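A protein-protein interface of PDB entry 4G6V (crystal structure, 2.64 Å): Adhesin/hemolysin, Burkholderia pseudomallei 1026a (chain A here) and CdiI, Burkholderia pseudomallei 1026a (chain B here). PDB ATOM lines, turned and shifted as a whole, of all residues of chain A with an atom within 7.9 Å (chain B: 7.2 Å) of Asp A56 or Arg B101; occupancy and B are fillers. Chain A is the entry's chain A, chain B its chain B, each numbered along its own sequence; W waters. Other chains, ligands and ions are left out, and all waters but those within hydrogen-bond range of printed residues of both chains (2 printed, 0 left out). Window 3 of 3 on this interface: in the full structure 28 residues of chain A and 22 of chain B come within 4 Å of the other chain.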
ATOM      1  N   ILE A  51     -14.757 -33.206  19.341  1.00  0.00           N
ATOM      2  CA  ILE A  51     -13.375 -32.758  19.344  1.00  0.00           C
ATOM      3  C   ILE A  51     -12.501 -33.880  19.861  1.00  0.00           C
ATOM      4  O   ILE A  51     -12.714 -34.340  20.970  1.00  0.00           O
ATOM      5  CB  ILE A  51     -13.233 -31.500  20.215  1.00  0.00           C
ATOM      6  CG1 ILE A  51     -14.233 -30.450  19.720  1.00  0.00           C
ATOM      7  CG2 ILE A  51     -11.769 -30.980  20.234  1.00  0.00           C
ATOM      8  CD1 ILE A  51     -14.245 -29.203  20.511  1.00  0.00           C
ATOM      9  N   PRO A  52     -11.539 -34.346  19.038  1.00  0.00           N
ATOM     10  CA  PRO A  52     -10.625 -35.427  19.417  1.00  0.00           C
ATOM     11  C   PRO A  52      -9.721 -34.980  20.564  1.00  0.00           C
ATOM     12  O   PRO A  52      -9.148 -33.886  20.495  1.00  0.00           O
ATOM     13  CB  PRO A  52      -9.792 -35.654  18.143  1.00  0.00           C
ATOM     14  CG  PRO A  52     -10.623 -35.084  17.041  1.00  0.00           C
ATOM     15  CD  PRO A  52     -11.297 -33.897  17.654  1.00  0.00           C
ATOM     16  N   PRO A  53      -9.593 -35.827  21.600  1.00  0.00           N
ATOM     17  CA  PRO A  53      -8.866 -35.557  22.839  1.00  0.00           C
ATOM     18  C   PRO A  53      -7.468 -34.987  22.583  1.00  0.00           C
ATOM     19  O   PRO A  53      -7.039 -34.062  23.279  1.00  0.00           O
ATOM     20  CB  PRO A  53      -8.735 -36.944  23.467  1.00  0.00           C
ATOM     21  CG  PRO A  53      -9.789 -37.765  22.852  1.00  0.00           C
ATOM     22  CD  PRO A  53     -10.029 -37.231  21.504  1.00  0.00           C
ATOM     23  N   LEU A  54      -6.761 -35.536  21.599  1.00  0.00           N
ATOM     24  CA  LEU A  54      -5.362 -35.155  21.378  1.00  0.00           C
ATOM     25  C   LEU A  54      -5.160 -33.810  20.679  1.00  0.00           C
ATOM     26  O   LEU A  54      -4.073 -33.247  20.750  1.00  0.00           O
ATOM     27  CB  LEU A  54      -4.569 -36.269  20.682  1.00  0.00           C
ATOM     28  CG  LEU A  54      -4.316 -37.461  21.612  1.00  0.00           C
ATOM     29  CD1 LEU A  54      -3.569 -38.572  20.919  1.00  0.00           C
ATOM     30  CD2 LEU A  54      -3.581 -37.026  22.847  1.00  0.00           C
ATOM     31  N   SER A  55      -6.198 -33.292  20.039  1.00  0.00           N
ATOM     32  CA  SER A  55      -6.168 -31.936  19.511  1.00  0.00           C
ATOM     33  C   SER A  55      -5.627 -30.987  20.561  1.00  0.00           C
ATOM     34  O   SER A  55      -5.989 -31.075  21.726  1.00  0.00           O
ATOM     35  CB  SER A  55      -7.579 -31.462  19.099  1.00  0.00           C
ATOM     36  OG  SER A  55      -8.320 -32.486  18.454  1.00  0.00           O
ATOM     37  N   ASP A  56      -4.777 -30.067  20.129  1.00  0.00           N
ATOM     38  CA  ASP A  56      -4.142 -29.072  20.995  1.00  0.00           C
ATOM     39  C   ASP A  56      -5.064 -27.886  21.247  1.00  0.00           C
ATOM     40  O   ASP A  56      -6.224 -27.923  20.881  1.00  0.00           O
ATOM     41  CB  ASP A  56      -2.885 -28.553  20.314  1.00  0.00           C
ATOM     42  CG  ASP A  56      -3.143 -28.166  18.873  1.00  0.00           C
ATOM     43  OD1 ASP A  56      -3.674 -27.056  18.622  1.00  0.00           O
ATOM     44  OD2 ASP A  56      -2.854 -29.005  17.995  1.00  0.00           O
ATOM     45  N   GLU A  57      -4.532 -26.817  21.834  1.00  0.00           N
ATOM     46  CA  GLU A  57      -5.366 -25.694  22.249  1.00  0.00           C
ATOM     47  C   GLU A  57      -5.943 -24.912  21.085  1.00  0.00           C
ATOM     48  O   GLU A  57      -7.106 -24.530  21.117  1.00  0.00           O
ATOM     49  CB  GLU A  57      -4.628 -24.756  23.209  1.00  0.00           C
ATOM     50  CG  GLU A  57      -4.286 -25.386  24.568  1.00  0.00           C
ATOM     51  CD  GLU A  57      -3.130 -26.394  24.509  1.00  0.00           C
ATOM     52  OE1 GLU A  57      -2.240 -26.279  23.607  1.00  0.00           O
ATOM     53  OE2 GLU A  57      -3.128 -27.292  25.389  1.00  0.00           O
ATOM     54  N   VAL A  58      -5.124 -24.688  20.060  1.00  0.00           N
ATOM     55  CA  VAL A  58      -5.540 -23.985  18.849  1.00  0.00           C
ATOM     56  C   VAL A  58      -6.685 -24.693  18.099  1.00  0.00           C
ATOM     57  O   VAL A  58      -7.741 -24.092  17.838  1.00  0.00           O
ATOM     58  CB  VAL A  58      -4.356 -23.805  17.878  1.00  0.00           C
ATOM     59  CG1 VAL A  58      -4.841 -23.300  16.525  1.00  0.00           C
ATOM     60  CG2 VAL A  58      -3.301 -22.869  18.470  1.00  0.00           C
ATOM     61  N   THR A  59      -6.456 -25.956  17.732  1.00  0.00           N
ATOM     62  CA  THR A  59      -7.448 -26.783  17.030  1.00  0.00           C
ATOM     63  C   THR A  59      -8.700 -26.962  17.865  1.00  0.00           C
ATOM     64  O   THR A  59      -9.815 -26.766  17.368  1.00  0.00           O
ATOM     65  CB  THR A  59      -6.885 -28.173  16.659  1.00  0.00           C
ATOM     66  OG1 THR A  59      -5.954 -28.038  15.580  1.00  0.00           O
ATOM     67  CG2 THR A  59      -7.982 -29.114  16.235  1.00  0.00           C
ATOM     68  N   THR A  60      -8.514 -27.319  19.137  1.00  0.00           N
ATOM     69  CA  THR A  60      -9.625 -27.429  20.071  1.00  0.00           C
ATOM     70  C   THR A  60     -10.493 -26.166  20.088  1.00  0.00           C
ATOM     71  O   THR A  60     -11.715 -26.250  20.066  1.00  0.00           O
ATOM     72  CB  THR A  60      -9.136 -27.771  21.495  1.00  0.00           C
ATOM     73  OG1 THR A  60      -8.532 -29.066  21.486  1.00  0.00           O
ATOM     74  CG2 THR A  60     -10.304 -27.778  22.494  1.00  0.00           C
ATOM     75  N   ARG A  61      -9.860 -24.998  20.110  1.00  0.00           N
ATOM     76  CA  ARG A  61     -10.598 -23.749  20.187  1.00  0.00           C
ATOM     77  C   ARG A  61     -11.416 -23.479  18.922  1.00  0.00           C
ATOM     78  O   ARG A  61     -12.502 -22.918  19.003  1.00  0.00           O
ATOM     79  CB  ARG A  61      -9.654 -22.582  20.491  1.00  0.00           C
ATOM     80  CG  ARG A  61     -10.363 -21.263  20.766  1.00  0.00           C
ATOM     81  CD  ARG A  61      -9.436 -20.061  20.590  1.00  0.00           C
ATOM     82  NE  ARG A  61      -8.781 -20.055  19.274  1.00  0.00           N
ATOM     83  CZ  ARG A  61      -9.340 -19.622  18.139  1.00  0.00           C
ATOM     84  NH1 ARG A  61     -10.590 -19.146  18.129  1.00  0.00           N
ATOM     85  NH2 ARG A  61      -8.647 -19.664  17.003  1.00  0.00           N
ATOM     86  N   SER A  62     -10.901 -23.867  17.755  1.00  0.00           N
ATOM     87  CA  SER A  62     -11.664 -23.682  16.509  1.00  0.00           C
ATOM     88  C   SER A  62     -12.889 -24.586  16.444  1.00  0.00           C
ATOM     89  O   SER A  62     -13.923 -24.163  15.956  1.00  0.00           O
ATOM     90  CB  SER A  62     -10.810 -23.860  15.242  1.00  0.00           C
ATOM     91  OG  SER A  62      -9.985 -22.726  15.017  1.00  0.00           O
ATOM     92  N   LEU B   5      -5.244 -25.558   6.512  1.00  0.00           N
ATOM     93  CA  LEU B   5      -3.820 -25.259   6.557  1.00  0.00           C
ATOM     94  C   LEU B   5      -3.438 -24.442   5.318  1.00  0.00           C
ATOM     95  O   LEU B   5      -3.595 -24.892   4.178  1.00  0.00           O
ATOM     96  CB  LEU B   5      -3.007 -26.557   6.675  1.00  0.00           C
ATOM     97  CG  LEU B   5      -3.378 -27.426   7.896  1.00  0.00           C
ATOM     98  CD1 LEU B   5      -2.596 -28.731   7.964  1.00  0.00           C
ATOM     99  CD2 LEU B   5      -3.231 -26.658   9.210  1.00  0.00           C
ATOM    100  N   ALA B  72      -8.967 -34.348  13.327  1.00  0.00           N
ATOM    101  CA  ALA B  72      -8.472 -33.023  13.688  1.00  0.00           C
ATOM    102  C   ALA B  72      -7.190 -33.115  14.480  1.00  0.00           C
ATOM    103  O   ALA B  72      -6.436 -32.145  14.587  1.00  0.00           O
ATOM    104  CB  ALA B  72      -9.519 -32.259  14.494  1.00  0.00           C
ATOM    105  N   ASP B  73      -6.943 -34.287  15.048  1.00  0.00           N
ATOM    106  CA  ASP B  73      -5.743 -34.463  15.835  1.00  0.00           C
ATOM    107  C   ASP B  73      -4.542 -34.895  14.989  1.00  0.00           C
ATOM    108  O   ASP B  73      -3.466 -35.142  15.528  1.00  0.00           O
ATOM    109  CB  ASP B  73      -5.983 -35.431  16.996  1.00  0.00           C
ATOM    110  CG  ASP B  73      -6.392 -36.828  16.531  1.00  0.00           C
ATOM    111  OD1 ASP B  73      -7.085 -36.962  15.464  1.00  0.00           O
ATOM    112  OD2 ASP B  73      -6.014 -37.787  17.262  1.00  0.00           O
ATOM    113  N   ILE B  75      -3.418 -32.928  12.490  1.00  0.00           N
ATOM    114  CA  ILE B  75      -2.856 -31.729  11.877  1.00  0.00           C
ATOM    115  C   ILE B  75      -1.326 -31.618  12.015  1.00  0.00           C
ATOM    116  O   ILE B  75      -0.645 -31.372  11.027  1.00  0.00           O
ATOM    117  CB  ILE B  75      -3.599 -30.448  12.323  1.00  0.00           C
ATOM    118  CG1 ILE B  75      -4.923 -30.344  11.569  1.00  0.00           C
ATOM    119  CG2 ILE B  75      -2.768 -29.213  12.087  1.00  0.00           C
ATOM    120  CD1 ILE B  75      -5.891 -29.270  12.107  1.00  0.00           C
ATOM    121  N   PRO B  76      -0.779 -31.827  13.225  1.00  0.00           N
ATOM    122  CA  PRO B  76       0.677 -31.773  13.430  1.00  0.00           C
ATOM    123  C   PRO B  76       1.452 -32.852  12.679  1.00  0.00           C
ATOM    124  O   PRO B  76       2.608 -32.623  12.298  1.00  0.00           O
ATOM    125  CB  PRO B  76       0.832 -32.010  14.943  1.00  0.00           C
ATOM    126  CG  PRO B  76      -0.474 -31.694  15.526  1.00  0.00           C
ATOM    127  CD  PRO B  76      -1.500 -32.044  14.491  1.00  0.00           C
ATOM    128  N   SER B  79       1.209 -31.780   9.015  1.00  0.00           N
ATOM    129  CA  SER B  79       2.144 -30.674   8.821  1.00  0.00           C
ATOM    130  C   SER B  79       3.553 -31.172   8.590  1.00  0.00           C
ATOM    131  O   SER B  79       4.253 -30.704   7.692  1.00  0.00           O
ATOM    132  CB  SER B  79       2.121 -29.737  10.016  1.00  0.00           C
ATOM    133  OG  SER B  79       0.886 -29.058  10.054  1.00  0.00           O
ATOM    134  N   LYS B  80       3.971 -32.129   9.410  1.00  0.00           N
ATOM    135  CA  LYS B  80       5.311 -32.698   9.306  1.00  0.00           C
ATOM    136  C   LYS B  80       5.504 -33.431   7.968  1.00  0.00           C
ATOM    137  O   LYS B  80       6.510 -33.234   7.295  1.00  0.00           O
ATOM    138  CB  LYS B  80       5.587 -33.610  10.504  1.00  0.00           C
ATOM    139  CG  LYS B  80       6.763 -34.517  10.309  1.00  0.00           C
ATOM    140  CD  LYS B  80       6.488 -35.906  10.860  1.00  0.00           C
ATOM    141  CE  LYS B  80       7.065 -36.994   9.946  1.00  0.00           C
ATOM    142  NZ  LYS B  80       8.540 -36.870   9.734  1.00  0.00           N
ATOM    143  N   VAL B  83       6.217 -30.721   5.368  1.00  0.00           N
ATOM    144  CA  VAL B  83       7.581 -30.193   5.482  1.00  0.00           C
ATOM    145  C   VAL B  83       8.609 -31.154   4.845  1.00  0.00           C
ATOM    146  O   VAL B  83       9.609 -30.725   4.243  1.00  0.00           O
ATOM    147  CB  VAL B  83       7.963 -29.956   6.991  1.00  0.00           C
ATOM    148  CG1 VAL B  83       9.446 -29.631   7.150  1.00  0.00           C
ATOM    149  CG2 VAL B  83       7.102 -28.877   7.652  1.00  0.00           C
ATOM    150  N   LEU B  92       6.030 -22.702   4.684  1.00  0.00           N
ATOM    151  CA  LEU B  92       5.433 -22.132   5.884  1.00  0.00           C
ATOM    152  C   LEU B  92       4.016 -22.688   5.961  1.00  0.00           C
ATOM    153  O   LEU B  92       3.312 -22.705   4.953  1.00  0.00           O
ATOM    154  CB  LEU B  92       5.436 -20.604   5.790  1.00  0.00           C
ATOM    155  CG  LEU B  92       4.441 -19.806   6.629  1.00  0.00           C
ATOM    156  CD1 LEU B  92       4.816 -19.903   8.069  1.00  0.00           C
ATOM    157  CD2 LEU B  92       4.404 -18.360   6.181  1.00  0.00           C
ATOM    158  N   ILE B  93       3.603 -23.183   7.123  1.00  0.00           N
ATOM    159  CA  ILE B  93       2.219 -23.657   7.285  1.00  0.00           C
ATOM    160  C   ILE B  93       1.477 -22.893   8.374  1.00  0.00           C
ATOM    161  O   ILE B  93       1.815 -23.005   9.546  1.00  0.00           O
ATOM    162  CB  ILE B  93       2.144 -25.158   7.650  1.00  0.00           C
ATOM    163  CG1 ILE B  93       2.817 -26.025   6.584  1.00  0.00           C
ATOM    164  CG2 ILE B  93       0.682 -25.580   7.872  1.00  0.00           C
ATOM    165  CD1 ILE B  93       2.795 -27.515   6.923  1.00  0.00           C
ATOM    166  N   LEU B  94       0.467 -22.129   7.990  1.00  0.00           N
ATOM    167  CA  LEU B  94      -0.362 -21.438   8.960  1.00  0.00           C
ATOM    168  C   LEU B  94      -1.777 -22.050   9.040  1.00  0.00           C
ATOM    169  O   LEU B  94      -2.572 -22.003   8.090  1.00  0.00           O
ATOM    170  CB  LEU B  94      -0.440 -19.945   8.634  1.00  0.00           C
ATOM    171  CG  LEU B  94       0.845 -19.136   8.489  1.00  0.00           C
ATOM    172  CD1 LEU B  94       0.531 -17.671   8.297  1.00  0.00           C
ATOM    173  CD2 LEU B  94       1.726 -19.294   9.704  1.00  0.00           C
ATOM    174  N   GLN B  95      -2.102 -22.632  10.185  1.00  0.00           N
ATOM    175  CA  GLN B  95      -3.449 -23.121  10.384  1.00  0.00           C
ATOM    176  C   GLN B  95      -4.382 -21.914  10.362  1.00  0.00           C
ATOM    177  O   GLN B  95      -4.174 -20.937  11.107  1.00  0.00           O
ATOM    178  CB  GLN B  95      -3.553 -23.859  11.697  1.00  0.00           C
ATOM    179  CG  GLN B  95      -4.818 -24.647  11.823  1.00  0.00           C
ATOM    180  CD  GLN B  95      -4.720 -25.737  12.860  1.00  0.00           C
ATOM    181  OE1 GLN B  95      -3.641 -26.282  13.111  1.00  0.00           O
ATOM    182  NE2 GLN B  95      -5.849 -26.068  13.465  1.00  0.00           N
ATOM    183  N   GLU B  98      -3.291 -18.205  10.449  1.00  0.00           N
ATOM    184  CA  GLU B  98      -3.030 -17.502  11.713  1.00  0.00           C
ATOM    185  C   GLU B  98      -1.918 -18.126  12.535  1.00  0.00           C
ATOM    186  O   GLU B  98      -0.998 -17.434  12.953  1.00  0.00           O
ATOM    187  CB  GLU B  98      -4.288 -17.451  12.588  1.00  0.00           C
ATOM    188  CG  GLU B  98      -5.329 -16.500  12.067  1.00  0.00           C
ATOM    189  CD  GLU B  98      -6.580 -16.464  12.907  1.00  0.00           C
ATOM    190  OE1 GLU B  98      -7.589 -15.948  12.393  1.00  0.00           O
ATOM    191  OE2 GLU B  98      -6.569 -16.944  14.057  1.00  0.00           O
ATOM    192  N   TYR B  99      -2.027 -19.430  12.769  1.00  0.00           N
ATOM    193  CA  TYR B  99      -1.146 -20.139  13.688  1.00  0.00           C
ATOM    194  C   TYR B  99      -0.020 -20.943  13.004  1.00  0.00           C
ATOM    195  O   TYR B  99      -0.275 -21.932  12.321  1.00  0.00           O
ATOM    196  CB  TYR B  99      -1.991 -21.053  14.583  1.00  0.00           C
ATOM    197  CG  TYR B  99      -1.188 -21.817  15.615  1.00  0.00           C
ATOM    198  CD1 TYR B  99      -1.073 -23.202  15.549  1.00  0.00           C
ATOM    199  CD2 TYR B  99      -0.540 -21.150  16.655  1.00  0.00           C
ATOM    200  CE1 TYR B  99      -0.346 -23.906  16.510  1.00  0.00           C
ATOM    201  CE2 TYR B  99       0.185 -21.843  17.608  1.00  0.00           C
ATOM    202  CZ  TYR B  99       0.283 -23.220  17.528  1.00  0.00           C
ATOM    203  OH  TYR B  99       1.022 -23.914  18.458  1.00  0.00           O
ATOM    204  N   ARG B 100       1.223 -20.536  13.220  1.00  0.00           N
ATOM    205  CA  ARG B 100       2.354 -21.216  12.583  1.00  0.00           C
ATOM    206  C   ARG B 100       2.557 -22.632  13.101  1.00  0.00           C
ATOM    207  O   ARG B 100       2.789 -22.831  14.292  1.00  0.00           O
ATOM    208  CB  ARG B 100       3.649 -20.425  12.742  1.00  0.00           C
ATOM    209  CG  ARG B 100       4.827 -21.123  12.093  1.00  0.00           C
ATOM    210  CD  ARG B 100       6.098 -20.254  12.129  1.00  0.00           C
ATOM    211  NE  ARG B 100       6.237 -19.505  13.374  1.00  0.00           N
ATOM    212  CZ  ARG B 100       6.854 -19.963  14.470  1.00  0.00           C
ATOM    213  NH1 ARG B 100       7.391 -21.173  14.476  1.00  0.00           N
ATOM    214  NH2 ARG B 100       6.930 -19.219  15.576  1.00  0.00           N
ATOM    215  N   ARG B 101       2.452 -23.613  12.207  1.00  0.00           N
ATOM    216  CA  ARG B 101       2.667 -25.008  12.572  1.00  0.00           C
ATOM    217  C   ARG B 101       4.064 -25.464  12.216  1.00  0.00           C
ATOM    218  O   ARG B 101       4.444 -26.594  12.495  1.00  0.00           O
ATOM    219  CB  ARG B 101       1.666 -25.905  11.876  1.00  0.00           C
ATOM    220  CG  ARG B 101       0.267 -25.791  12.410  1.00  0.00           C
ATOM    221  CD  ARG B 101       0.029 -26.825  13.484  1.00  0.00           C
ATOM    222  NE  ARG B 101      -1.334 -26.764  14.000  1.00  0.00           N
ATOM    223  CZ  ARG B 101      -1.661 -27.054  15.256  1.00  0.00           C
ATOM    224  NH1 ARG B 101      -0.726 -27.414  16.130  1.00  0.00           N
ATOM    225  NH2 ARG B 101      -2.921 -26.973  15.648  1.00  0.00           N
ATOM    226  N   THR B 102       4.831 -24.587  11.587  1.00  0.00           N
ATOM    227  CA  THR B 102       6.165 -24.956  11.158  1.00  0.00           C
ATOM    228  C   THR B 102       7.228 -24.163  11.896  1.00  0.00           C
ATOM    229  O   THR B 102       6.947 -23.120  12.486  1.00  0.00           O
ATOM    230  CB  THR B 102       6.372 -24.717   9.672  1.00  0.00           C
ATOM    231  OG1 THR B 102       5.898 -23.407   9.340  1.00  0.00           O
ATOM    232  CG2 THR B 102       5.664 -25.787   8.850  1.00  0.00           C
ATOM    233  N   SER B 103       8.458 -24.653  11.832  1.00  0.00           N
ATOM    234  CA  SER B 103       9.554 -24.021  12.539  1.00  0.00           C
ATOM    235  C   SER B 103      10.011 -22.701  11.923  1.00  0.00           C
ATOM    236  O   SER B 103      10.201 -22.597  10.726  1.00  0.00           O
ATOM    237  CB  SER B 103      10.717 -25.006  12.666  1.00  0.00           C
ATOM    238  OG  SER B 103      10.399 -25.974  13.659  1.00  0.00           O
ATOM    239  N   LEU B 104      10.141 -21.696  12.780  1.00  0.00           N
ATOM    240  CA  LEU B 104      10.802 -20.410  12.500  1.00  0.00           C
ATOM    241  C   LEU B 104       9.943 -19.384  11.773  1.00  0.00           C
ATOM    242  O   LEU B 104       9.823 -18.244  12.238  1.00  0.00           O
ATOM    243  CB  LEU B 104      12.251 -20.589  11.848  1.00  0.00           C
HETATM  244  O   HOH W   1      -4.624 -30.569  15.818  1.00  0.00           O
HETATM  245  O   HOH W   2      -7.515 -37.729  20.002  1.00  0.00           O
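Among the printed residues, pairs that only touch across the chains: Thr A59 with Ile B75 (3.7 Å), Val A58 with Tyr B99 (3.7 Å), Ser A55 with Asp B73 (3.7 Å), Thr A59 with Ala B72 (3.8 Å), Pro A52 with Asp B73 (3.9 Å) and Pro A52 with Ala B72 (3.96 Å).
Printed residues of chain B that touch a printed residue of chain A: Ala B72, Asp B73, Ile B75, Gln B95, Tyr B99 and Arg B101.
Hydrophobic or aromatic side chains of chain A within 4 Å of the printed part of chain B: Pro A52 and Val A58.
Among the printed residues, Asp or Glu carboxylates within 4 Å of a Lys or Arg side-chain nitrogen of the other chain: Asp A56 with Arg B101.
Of chain B, only Arg B101 comes within 4 Å of Asp A56.
Of the printed residues of chain A, Arg B101 touches Asp A56 (3.1 Å) and Thr A59 (3.2 Å).
Of the printed residues of chain B, Pro A52 touches Ala B72 (3.96 Å) and Asp B73 (3.9 Å).
Of the printed residues of chain A, Tyr B99 touches Val A58.
Of the printed residues of chain B, Ser A55 touches Asp B73 (3.7 Å).
Of the printed residues of chain A, Ala B72 touches Pro A52 (3.96 Å) and Thr A59 (3.8 Å).
Of the printed residues of chain A, Ile B75 touches Thr A59 (3.7 Å).
The nearest printed residue of chain A that does not touch Ala B72 is Ser A55 (4.1 Å).
The guanidinium group of Arg B101 is in salt-bridge range of the side-chain carboxylate of Asp A56 (3.1 Å).
NE2 of Gln B95 lies within hydrogen-bond range of OG1 of Thr A59 (2.9 Å).
OG1 of Thr A59 lies within hydrogen-bond range of NH2 of Arg B101 (3.2 Å).
The backbone NH (N) of Val A58 is in hydrogen-bond range of the side-chain carboxylate (OD1) of Asp A56 (3.1 Å).
The backbone carbonyl oxygen of Asp A56 sits at hydrogen-bond distance from the side-chain hydroxyl of Thr A60, 2.6 Å away.
The side-chain carboxylate of Asp A56 lies within hydrogen-bond range of the backbone NH of Thr A59 (3.1 Å).
The backbone carbonyl oxygen (O) of Ser A55 sits at hydrogen-bond distance from the side-chain hydroxyl (OG1) of Thr A60 (3.2 Å).
O of Pro A52 sits at hydrogen-bond distance from OG of Ser A55, at 2.6 Å.
N of Arg B101 is in hydrogen-bond range of O of Ile B93, at 2.8 Å.
Water W1 lies within hydrogen-bond range of O of Ala B72, OG1 of Thr A59 and OD2 of Asp A56.
Water W2 bridges N of Leu A54 and OD2 of Asp B73.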
